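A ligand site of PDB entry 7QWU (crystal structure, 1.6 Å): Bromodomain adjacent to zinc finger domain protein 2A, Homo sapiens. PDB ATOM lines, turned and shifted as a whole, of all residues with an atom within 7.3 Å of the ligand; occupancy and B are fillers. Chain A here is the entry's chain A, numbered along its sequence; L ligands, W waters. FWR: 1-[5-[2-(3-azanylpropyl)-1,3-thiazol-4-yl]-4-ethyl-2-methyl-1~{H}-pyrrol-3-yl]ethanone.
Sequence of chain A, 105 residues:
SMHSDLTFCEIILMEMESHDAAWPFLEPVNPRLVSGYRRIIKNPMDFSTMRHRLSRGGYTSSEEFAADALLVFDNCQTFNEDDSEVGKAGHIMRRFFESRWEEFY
O of Pro 24 is in hydrogen-bond range of N05 of the ligand.
ND2 of Asn 80 sits at hydrogen-bond distance from O10 of the ligand, 2.9 Å away.
ND2 of Asn 80 is in hydrogen-bond range of O of Cys 76 (3.1 Å).
The side-chain sulfur of Cys 76 is in hydrogen-bond range of the backbone carbonyl oxygen of Val 86 (3.4 Å).
CZ3 of Trp 23 touches S14 of the ligand, 3.8 Å away.
CG2 of Val 29 touches C07 of the ligand (3.6 Å).
CG1 of Val 34 touches C11 of the ligand, 3.9 Å away.
Tyr 37 touches the ligand (CE1 to O10, 3.7 Å).
Phe 79 touches the ligand (CD2 to C11, 3.6 Å).
CG2 of Val 86 touches C01 of the ligand, at 3.6 Å.
The nearest printed residue that does not touch the ligand is Phe 25 (4.03 Å).
Water W2 lies within hydrogen-bond range of O of Pro 24 (2.9 Å), N20 of the ligand (2.9 Å) and O of Glu 27 (3.4 Å).
Water W1 lies within hydrogen-bond range of the side-chain hydroxyl of Tyr 37 (2.5 Å), an oxygen (O10) of the ligand (3.0 Å) and the backbone NH of Cys 76 (3.3 Å).
Water W3 lies within hydrogen-bond range of the backbone carbonyl oxygen of Trp 23, a nitrogen (N19) of the ligand, the backbone NH of Leu 26 and the backbone NH of Glu 27.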
ATOM      1  N   ALA A  22      -9.093  -9.890  -7.418  1.00  0.00           N
ATOM      2  CA  ALA A  22      -7.855 -10.646  -7.571  1.00  0.00           C
ATOM      3  C   ALA A  22      -7.257 -11.099  -6.254  1.00  0.00           C
ATOM      4  O   ALA A  22      -6.325 -11.920  -6.278  1.00  0.00           O
ATOM      5  CB  ALA A  22      -6.812  -9.810  -8.310  1.00  0.00           C
ATOM      6  N   TRP A  23      -7.765 -10.619  -5.134  1.00  0.00           N
ATOM      7  CA  TRP A  23      -7.128 -10.815  -3.836  1.00  0.00           C
ATOM      8  C   TRP A  23      -6.818 -12.276  -3.471  1.00  0.00           C
ATOM      9  O   TRP A  23      -5.797 -12.498  -2.792  1.00  0.00           O
ATOM     10  CB  TRP A  23      -7.969 -10.178  -2.723  1.00  0.00           C
ATOM     11  CG  TRP A  23      -9.365 -10.661  -2.610  1.00  0.00           C
ATOM     12  CD1 TRP A  23     -10.473 -10.149  -3.224  1.00  0.00           C
ATOM     13  CD2 TRP A  23      -9.820 -11.767  -1.820  1.00  0.00           C
ATOM     14  NE1 TRP A  23     -11.590 -10.873  -2.871  1.00  0.00           N
ATOM     15  CE2 TRP A  23     -11.215 -11.876  -2.016  1.00  0.00           C
ATOM     16  CE3 TRP A  23      -9.191 -12.694  -0.985  1.00  0.00           C
ATOM     17  CZ2 TRP A  23     -11.980 -12.854  -1.408  1.00  0.00           C
ATOM     18  CZ3 TRP A  23      -9.959 -13.662  -0.375  1.00  0.00           C
ATOM     19  CH2 TRP A  23     -11.338 -13.743  -0.585  1.00  0.00           C
ATOM     20  N   PRO A  24      -7.600 -13.283  -3.862  1.00  0.00           N
ATOM     21  CA  PRO A  24      -7.229 -14.666  -3.486  1.00  0.00           C
ATOM     22  C   PRO A  24      -6.082 -15.222  -4.277  1.00  0.00           C
ATOM     23  O   PRO A  24      -5.548 -16.273  -3.905  1.00  0.00           O
ATOM     24  CB  PRO A  24      -8.508 -15.473  -3.779  1.00  0.00           C
ATOM     25  CG  PRO A  24      -9.597 -14.483  -3.976  1.00  0.00           C
ATOM     26  CD  PRO A  24      -8.917 -13.283  -4.551  1.00  0.00           C
ATOM     27  N   PHE A  25      -5.692 -14.561  -5.371  1.00  0.00           N
ATOM     28  CA  PHE A  25      -4.845 -15.146  -6.403  1.00  0.00           C
ATOM     29  C   PHE A  25      -3.484 -14.494  -6.519  1.00  0.00           C
ATOM     30  O   PHE A  25      -2.705 -14.868  -7.406  1.00  0.00           O
ATOM     31  CB  PHE A  25      -5.574 -15.097  -7.738  1.00  0.00           C
ATOM     32  CG  PHE A  25      -6.968 -15.606  -7.661  1.00  0.00           C
ATOM     33  CD1 PHE A  25      -7.218 -16.923  -7.297  1.00  0.00           C
ATOM     34  CD2 PHE A  25      -8.046 -14.755  -7.892  1.00  0.00           C
ATOM     35  CE1 PHE A  25      -8.515 -17.405  -7.215  1.00  0.00           C
ATOM     36  CE2 PHE A  25      -9.336 -15.224  -7.807  1.00  0.00           C
ATOM     37  CZ  PHE A  25      -9.579 -16.556  -7.476  1.00  0.00           C
ATOM     38  N   LEU A  26      -3.145 -13.566  -5.627  1.00  0.00           N
ATOM     39  CA  LEU A  26      -1.921 -12.798  -5.796  1.00  0.00           C
ATOM     40  C   LEU A  26      -0.683 -13.611  -5.439  1.00  0.00           C
ATOM     41  O   LEU A  26       0.381 -13.412  -6.038  1.00  0.00           O
ATOM     42  CB  LEU A  26      -1.998 -11.515  -4.984  1.00  0.00           C
ATOM     43  CG  LEU A  26      -3.255 -10.707  -5.273  1.00  0.00           C
ATOM     44  CD1 LEU A  26      -3.369  -9.575  -4.298  1.00  0.00           C
ATOM     45  CD2 LEU A  26      -3.269 -10.184  -6.700  1.00  0.00           C
ATOM     46  N   GLU A  27      -0.767 -14.521  -4.482  1.00  0.00           N
ATOM     47  CA  GLU A  27       0.363 -15.308  -4.019  1.00  0.00           C
ATOM     48  C   GLU A  27      -0.042 -16.769  -3.902  1.00  0.00           C
ATOM     49  O   GLU A  27      -1.242 -17.079  -3.860  1.00  0.00           O
ATOM     50  CB  GLU A  27       0.894 -14.775  -2.668  1.00  0.00           C
ATOM     51  CG  GLU A  27       2.375 -14.384  -2.707  1.00  0.00           C
ATOM     52  CD  GLU A  27       2.620 -12.919  -2.400  1.00  0.00           C
ATOM     53  OE1 GLU A  27       2.371 -12.485  -1.252  1.00  0.00           O
ATOM     54  OE2 GLU A  27       3.071 -12.195  -3.313  1.00  0.00           O
ATOM     55  N   PRO A  28       0.918 -17.699  -3.851  1.00  0.00           N
ATOM     56  CA  PRO A  28       0.555 -19.115  -3.742  1.00  0.00           C
ATOM     57  C   PRO A  28      -0.236 -19.392  -2.476  1.00  0.00           C
ATOM     58  O   PRO A  28      -0.016 -18.776  -1.429  1.00  0.00           O
ATOM     59  CB  PRO A  28       1.909 -19.824  -3.712  1.00  0.00           C
ATOM     60  CG  PRO A  28       2.839 -18.913  -4.397  1.00  0.00           C
ATOM     61  CD  PRO A  28       2.382 -17.540  -3.986  1.00  0.00           C
ATOM     62  N   VAL A  29      -1.160 -20.335  -2.593  1.00  0.00           N
ATOM     63  CA  VAL A  29      -1.961 -20.746  -1.434  1.00  0.00           C
ATOM     64  C   VAL A  29      -1.047 -21.428  -0.422  1.00  0.00           C
ATOM     65  O   VAL A  29      -0.222 -22.282  -0.780  1.00  0.00           O
ATOM     66  CB  VAL A  29      -3.099 -21.692  -1.861  1.00  0.00           C
ATOM     67  CG1 VAL A  29      -3.860 -22.203  -0.655  1.00  0.00           C
ATOM     68  CG2 VAL A  29      -4.053 -20.994  -2.844  1.00  0.00           C
ATOM     69  N   ASN A  30      -1.205 -21.048   0.838  1.00  0.00           N
ATOM     70  CA  ASN A  30      -0.323 -21.516   1.896  1.00  0.00           C
ATOM     71  C   ASN A  30      -0.853 -22.837   2.445  1.00  0.00           C
ATOM     72  O   ASN A  30      -1.923 -22.861   3.055  1.00  0.00           O
ATOM     73  CB  ASN A  30      -0.268 -20.472   3.005  1.00  0.00           C
ATOM     74  CG  ASN A  30       0.910 -20.675   3.929  1.00  0.00           C
ATOM     75  OD1 ASN A  30       1.330 -21.812   4.171  1.00  0.00           O
ATOM     76  ND2 ASN A  30       1.438 -19.587   4.472  1.00  0.00           N
ATOM     77  N   LEU A  33      -2.162 -22.885   5.949  1.00  0.00           N
ATOM     78  CA  LEU A  33      -3.419 -22.162   6.146  1.00  0.00           C
ATOM     79  C   LEU A  33      -4.612 -22.847   5.496  1.00  0.00           C
ATOM     80  O   LEU A  33      -5.743 -22.535   5.855  1.00  0.00           O
ATOM     81  CB  LEU A  33      -3.302 -20.736   5.584  1.00  0.00           C
ATOM     82  CG  LEU A  33      -2.226 -19.900   6.260  1.00  0.00           C
ATOM     83  CD1 LEU A  33      -2.293 -18.470   5.802  1.00  0.00           C
ATOM     84  CD2 LEU A  33      -2.375 -19.977   7.774  1.00  0.00           C
ATOM     85  N   VAL A  34      -4.383 -23.748   4.535  1.00  0.00           N
ATOM     86  CA  VAL A  34      -5.458 -24.410   3.820  1.00  0.00           C
ATOM     87  C   VAL A  34      -5.137 -25.895   3.814  1.00  0.00           C
ATOM     88  O   VAL A  34      -4.299 -26.351   3.020  1.00  0.00           O
ATOM     89  CB  VAL A  34      -5.627 -23.889   2.386  1.00  0.00           C
ATOM     90  CG1 VAL A  34      -6.842 -24.556   1.778  1.00  0.00           C
ATOM     91  CG2 VAL A  34      -5.826 -22.376   2.369  1.00  0.00           C
ATOM     92  N   TYR A  37      -4.504 -28.518   0.736  1.00  0.00           N
ATOM     93  CA  TYR A  37      -4.710 -27.833  -0.538  1.00  0.00           C
ATOM     94  C   TYR A  37      -3.865 -28.450  -1.638  1.00  0.00           C
ATOM     95  O   TYR A  37      -4.372 -28.799  -2.706  1.00  0.00           O
ATOM     96  CB  TYR A  37      -4.418 -26.344  -0.437  1.00  0.00           C
ATOM     97  CG  TYR A  37      -4.650 -25.648  -1.764  1.00  0.00           C
ATOM     98  CD1 TYR A  37      -5.948 -25.326  -2.177  1.00  0.00           C
ATOM     99  CD2 TYR A  37      -3.604 -25.379  -2.637  1.00  0.00           C
ATOM    100  CE1 TYR A  37      -6.181 -24.719  -3.408  1.00  0.00           C
ATOM    101  CE2 TYR A  37      -3.838 -24.771  -3.868  1.00  0.00           C
ATOM    102  CZ  TYR A  37      -5.132 -24.445  -4.239  1.00  0.00           C
ATOM    103  OH  TYR A  37      -5.354 -23.847  -5.460  1.00  0.00           O
ATOM    104  N   ILE A  41      -4.927 -30.205  -5.120  1.00  0.00           N
ATOM    105  CA  ILE A  41      -4.554 -29.460  -6.313  1.00  0.00           C
ATOM    106  C   ILE A  41      -3.111 -29.812  -6.657  1.00  0.00           C
ATOM    107  O   ILE A  41      -2.174 -29.348  -6.003  1.00  0.00           O
ATOM    108  CB  ILE A  41      -4.706 -27.951  -6.081  1.00  0.00           C
ATOM    109  CG1 ILE A  41      -6.155 -27.625  -5.722  1.00  0.00           C
ATOM    110  CG2 ILE A  41      -4.225 -27.173  -7.287  1.00  0.00           C
ATOM    111  CD1 ILE A  41      -7.145 -27.994  -6.813  1.00  0.00           C
ATOM    112  N   MET A  45      -1.258 -22.553  -8.903  1.00  0.00           N
ATOM    113  CA  MET A  45      -0.822 -21.453  -9.758  1.00  0.00           C
ATOM    114  C   MET A  45      -1.413 -20.159  -9.222  1.00  0.00           C
ATOM    115  O   MET A  45      -2.522 -20.151  -8.692  1.00  0.00           O
ATOM    116  CB  MET A  45      -1.248 -21.688 -11.205  1.00  0.00           C
ATOM    117  CG  MET A  45      -0.689 -20.629 -12.178  1.00  0.00           C
ATOM    118  SD  MET A  45       1.090 -20.357 -12.044  1.00  0.00           S
ATOM    119  CE  MET A  45       1.674 -22.038 -12.335  1.00  0.00           C
ATOM    120  N   VAL A  72      -5.196 -21.052 -12.676  1.00  0.00           N
ATOM    121  CA  VAL A  72      -5.601 -20.348 -11.453  1.00  0.00           C
ATOM    122  C   VAL A  72      -7.096 -20.534 -11.204  1.00  0.00           C
ATOM    123  O   VAL A  72      -7.519 -20.851 -10.080  1.00  0.00           O
ATOM    124  CB  VAL A  72      -5.250 -18.854 -11.548  1.00  0.00           C
ATOM    125  CG1 VAL A  72      -5.814 -18.100 -10.333  1.00  0.00           C
ATOM    126  CG2 VAL A  72      -3.745 -18.650 -11.691  1.00  0.00           C
ATOM    127  N   ASN A  75      -8.207 -24.358 -10.729  1.00  0.00           N
ATOM    128  CA  ASN A  75      -7.894 -24.754  -9.359  1.00  0.00           C
ATOM    129  C   ASN A  75      -8.912 -24.199  -8.381  1.00  0.00           C
ATOM    130  O   ASN A  75      -9.404 -24.910  -7.491  1.00  0.00           O
ATOM    131  CB  ASN A  75      -6.495 -24.250  -8.987  1.00  0.00           C
ATOM    132  CG  ASN A  75      -5.386 -25.046  -9.662  1.00  0.00           C
ATOM    133  OD1 ASN A  75      -5.623 -26.123 -10.214  1.00  0.00           O
ATOM    134  ND2 ASN A  75      -4.172 -24.525  -9.613  1.00  0.00           N
ATOM    135  N   CYS A  76      -9.259 -22.917  -8.538  1.00  0.00           N
ATOM    136  CA  CYS A  76     -10.180 -22.264  -7.613  1.00  0.00           C
ATOM    137  C   CYS A  76     -11.537 -22.938  -7.624  1.00  0.00           C
ATOM    138  O   CYS A  76     -12.122 -23.239  -6.565  1.00  0.00           O
ATOM    139  CB  CYS A  76     -10.302 -20.786  -8.007  1.00  0.00           C
ATOM    140  SG  CYS A  76     -11.357 -19.808  -6.975  1.00  0.00           S
ATOM    141  N   GLN A  77     -12.049 -23.237  -8.817  1.00  0.00           N
ATOM    142  CA  GLN A  77     -13.329 -23.919  -8.974  1.00  0.00           C
ATOM    143  C   GLN A  77     -13.276 -25.358  -8.479  1.00  0.00           C
ATOM    144  O   GLN A  77     -14.295 -25.882  -8.018  1.00  0.00           O
ATOM    145  CB  GLN A  77     -13.725 -23.856 -10.456  1.00  0.00           C
ATOM    146  CG  GLN A  77     -15.175 -24.191 -10.720  1.00  0.00           C
ATOM    147  CD  GLN A  77     -15.522 -24.084 -12.189  1.00  0.00           C
ATOM    148  OE1 GLN A  77     -16.658 -24.339 -12.590  1.00  0.00           O
ATOM    149  NE2 GLN A  77     -14.542 -23.716 -13.010  1.00  0.00           N
ATOM    150  N   PHE A  79     -11.475 -26.343  -5.836  1.00  0.00           N
ATOM    151  CA  PHE A  79     -11.349 -26.365  -4.375  1.00  0.00           C
ATOM    152  C   PHE A  79     -12.423 -25.564  -3.664  1.00  0.00           C
ATOM    153  O   PHE A  79     -12.795 -25.920  -2.532  1.00  0.00           O
ATOM    154  CB  PHE A  79      -9.977 -25.823  -3.957  1.00  0.00           C
ATOM    155  CG  PHE A  79      -9.556 -26.243  -2.570  1.00  0.00           C
ATOM    156  CD1 PHE A  79      -8.792 -27.376  -2.393  1.00  0.00           C
ATOM    157  CD2 PHE A  79      -9.934 -25.492  -1.469  1.00  0.00           C
ATOM    158  CE1 PHE A  79      -8.413 -27.769  -1.118  1.00  0.00           C
ATOM    159  CE2 PHE A  79      -9.552 -25.895  -0.195  1.00  0.00           C
ATOM    160  CZ  PHE A  79      -8.787 -27.026  -0.028  1.00  0.00           C
ATOM    161  N   ASN A  80     -12.938 -24.493  -4.266  1.00  0.00           N
ATOM    162  CA  ASN A  80     -13.837 -23.586  -3.578  1.00  0.00           C
ATOM    163  C   ASN A  80     -15.282 -23.740  -4.054  1.00  0.00           C
ATOM    164  O   ASN A  80     -15.542 -24.010  -5.235  1.00  0.00           O
ATOM    165  CB  ASN A  80     -13.379 -22.131  -3.762  1.00  0.00           C
ATOM    166  CG  ASN A  80     -12.003 -21.869  -3.161  1.00  0.00           C
ATOM    167  OD1 ASN A  80     -11.864 -21.669  -1.954  1.00  0.00           O
ATOM    168  ND2 ASN A  80     -10.969 -21.894  -3.998  1.00  0.00           N
ATOM    169  N   SER A  84     -18.857 -19.307  -2.237  1.00  0.00           N
ATOM    170  CA  SER A  84     -17.867 -18.810  -1.295  1.00  0.00           C
ATOM    171  C   SER A  84     -17.254 -17.511  -1.809  1.00  0.00           C
ATOM    172  O   SER A  84     -17.374 -17.164  -2.984  1.00  0.00           O
ATOM    173  CB  SER A  84     -16.761 -19.840  -1.074  1.00  0.00           C
ATOM    174  OG  SER A  84     -15.965 -19.956  -2.239  1.00  0.00           O
ATOM    175  N   GLU A  85     -16.579 -16.795  -0.900  1.00  0.00           N
ATOM    176  CA  GLU A  85     -15.932 -15.538  -1.285  1.00  0.00           C
ATOM    177  C   GLU A  85     -14.880 -15.761  -2.372  1.00  0.00           C
ATOM    178  O   GLU A  85     -14.858 -15.061  -3.385  1.00  0.00           O
ATOM    179  CB  GLU A  85     -15.312 -14.875  -0.065  1.00  0.00           C
ATOM    180  CG  GLU A  85     -16.333 -14.169   0.808  1.00  0.00           C
ATOM    181  CD  GLU A  85     -17.233 -13.260  -0.007  1.00  0.00           C
ATOM    182  OE1 GLU A  85     -16.746 -12.214  -0.489  1.00  0.00           O
ATOM    183  OE2 GLU A  85     -18.424 -13.597  -0.184  1.00  0.00           O
ATOM    184  N   VAL A  86     -13.980 -16.725  -2.149  1.00  0.00           N
ATOM    185  CA  VAL A  86     -12.960 -17.033  -3.153  1.00  0.00           C
ATOM    186  C   VAL A  86     -13.595 -17.622  -4.402  1.00  0.00           C
ATOM    187  O   VAL A  86     -13.206 -17.294  -5.527  1.00  0.00           O
ATOM    188  CB  VAL A  86     -11.896 -17.968  -2.540  1.00  0.00           C
ATOM    189  CG1 VAL A  86     -10.927 -18.437  -3.620  1.00  0.00           C
ATOM    190  CG2 VAL A  86     -11.153 -17.260  -1.381  1.00  0.00           C
ATOM    191  N   GLY A  87     -14.579 -18.511  -4.229  1.00  0.00           N
ATOM    192  CA  GLY A  87     -15.267 -19.066  -5.396  1.00  0.00           C
ATOM    193  C   GLY A  87     -15.863 -17.994  -6.292  1.00  0.00           C
ATOM    194  O   GLY A  87     -15.687 -18.027  -7.517  1.00  0.00           O
HETATM  195  C01 FWR L   1      -9.825 -19.579   1.048  1.00  0.00           C
HETATM  196  C02 FWR L   1      -8.320 -19.748   0.867  1.00  0.00           C
HETATM  197  C03 FWR L   1      -7.801 -19.205  -0.450  1.00  0.00           C
HETATM  198  C04 FWR L   1      -7.288 -17.956  -0.697  1.00  0.00           C
HETATM  199  C06 FWR L   1      -7.225 -19.047  -2.569  1.00  0.00           C
HETATM  200  C07 FWR L   1      -6.970 -19.356  -4.041  1.00  0.00           C
HETATM  201  C08 FWR L   1      -7.742 -19.888  -1.634  1.00  0.00           C
HETATM  202  C09 FWR L   1      -8.190 -21.296  -1.941  1.00  0.00           C
HETATM  203  C11 FWR L   1      -8.588 -22.258  -0.821  1.00  0.00           C
HETATM  204  C12 FWR L   1      -7.099 -16.748   0.211  1.00  0.00           C
HETATM  205  C13 FWR L   1      -7.829 -16.402   1.374  1.00  0.00           C
HETATM  206  C15 FWR L   1      -6.129 -14.707   0.864  1.00  0.00           C
HETATM  207  C16 FWR L   1      -5.223 -13.496   0.845  1.00  0.00           C
HETATM  208  C17 FWR L   1      -3.785 -13.754   1.254  1.00  0.00           C
HETATM  209  C18 FWR L   1      -3.010 -12.446   1.311  1.00  0.00           C
HETATM  210  N05 FWR L   1      -6.959 -17.904  -1.982  1.00  0.00           N
HETATM  211  N19 FWR L   1      -3.009 -11.812   0.008  1.00  0.00           N
HETATM  212  N20 FWR L   1      -6.104 -15.723  -0.068  1.00  0.00           N
HETATM  213  O10 FWR L   1      -8.230 -21.652  -3.044  1.00  0.00           O
HETATM  214  S14 FWR L   1      -7.286 -14.999   1.957  1.00  0.00           S
HETATM  215  O   HOH W   1      -7.487 -22.504  -5.802  1.00  0.00           O
HETATM  216  O   HOH W   2      -3.679 -16.220  -1.655  1.00  0.00           O
HETATM  217  O   HOH W   3      -3.374 -13.744  -2.463  1.00  0.00           O
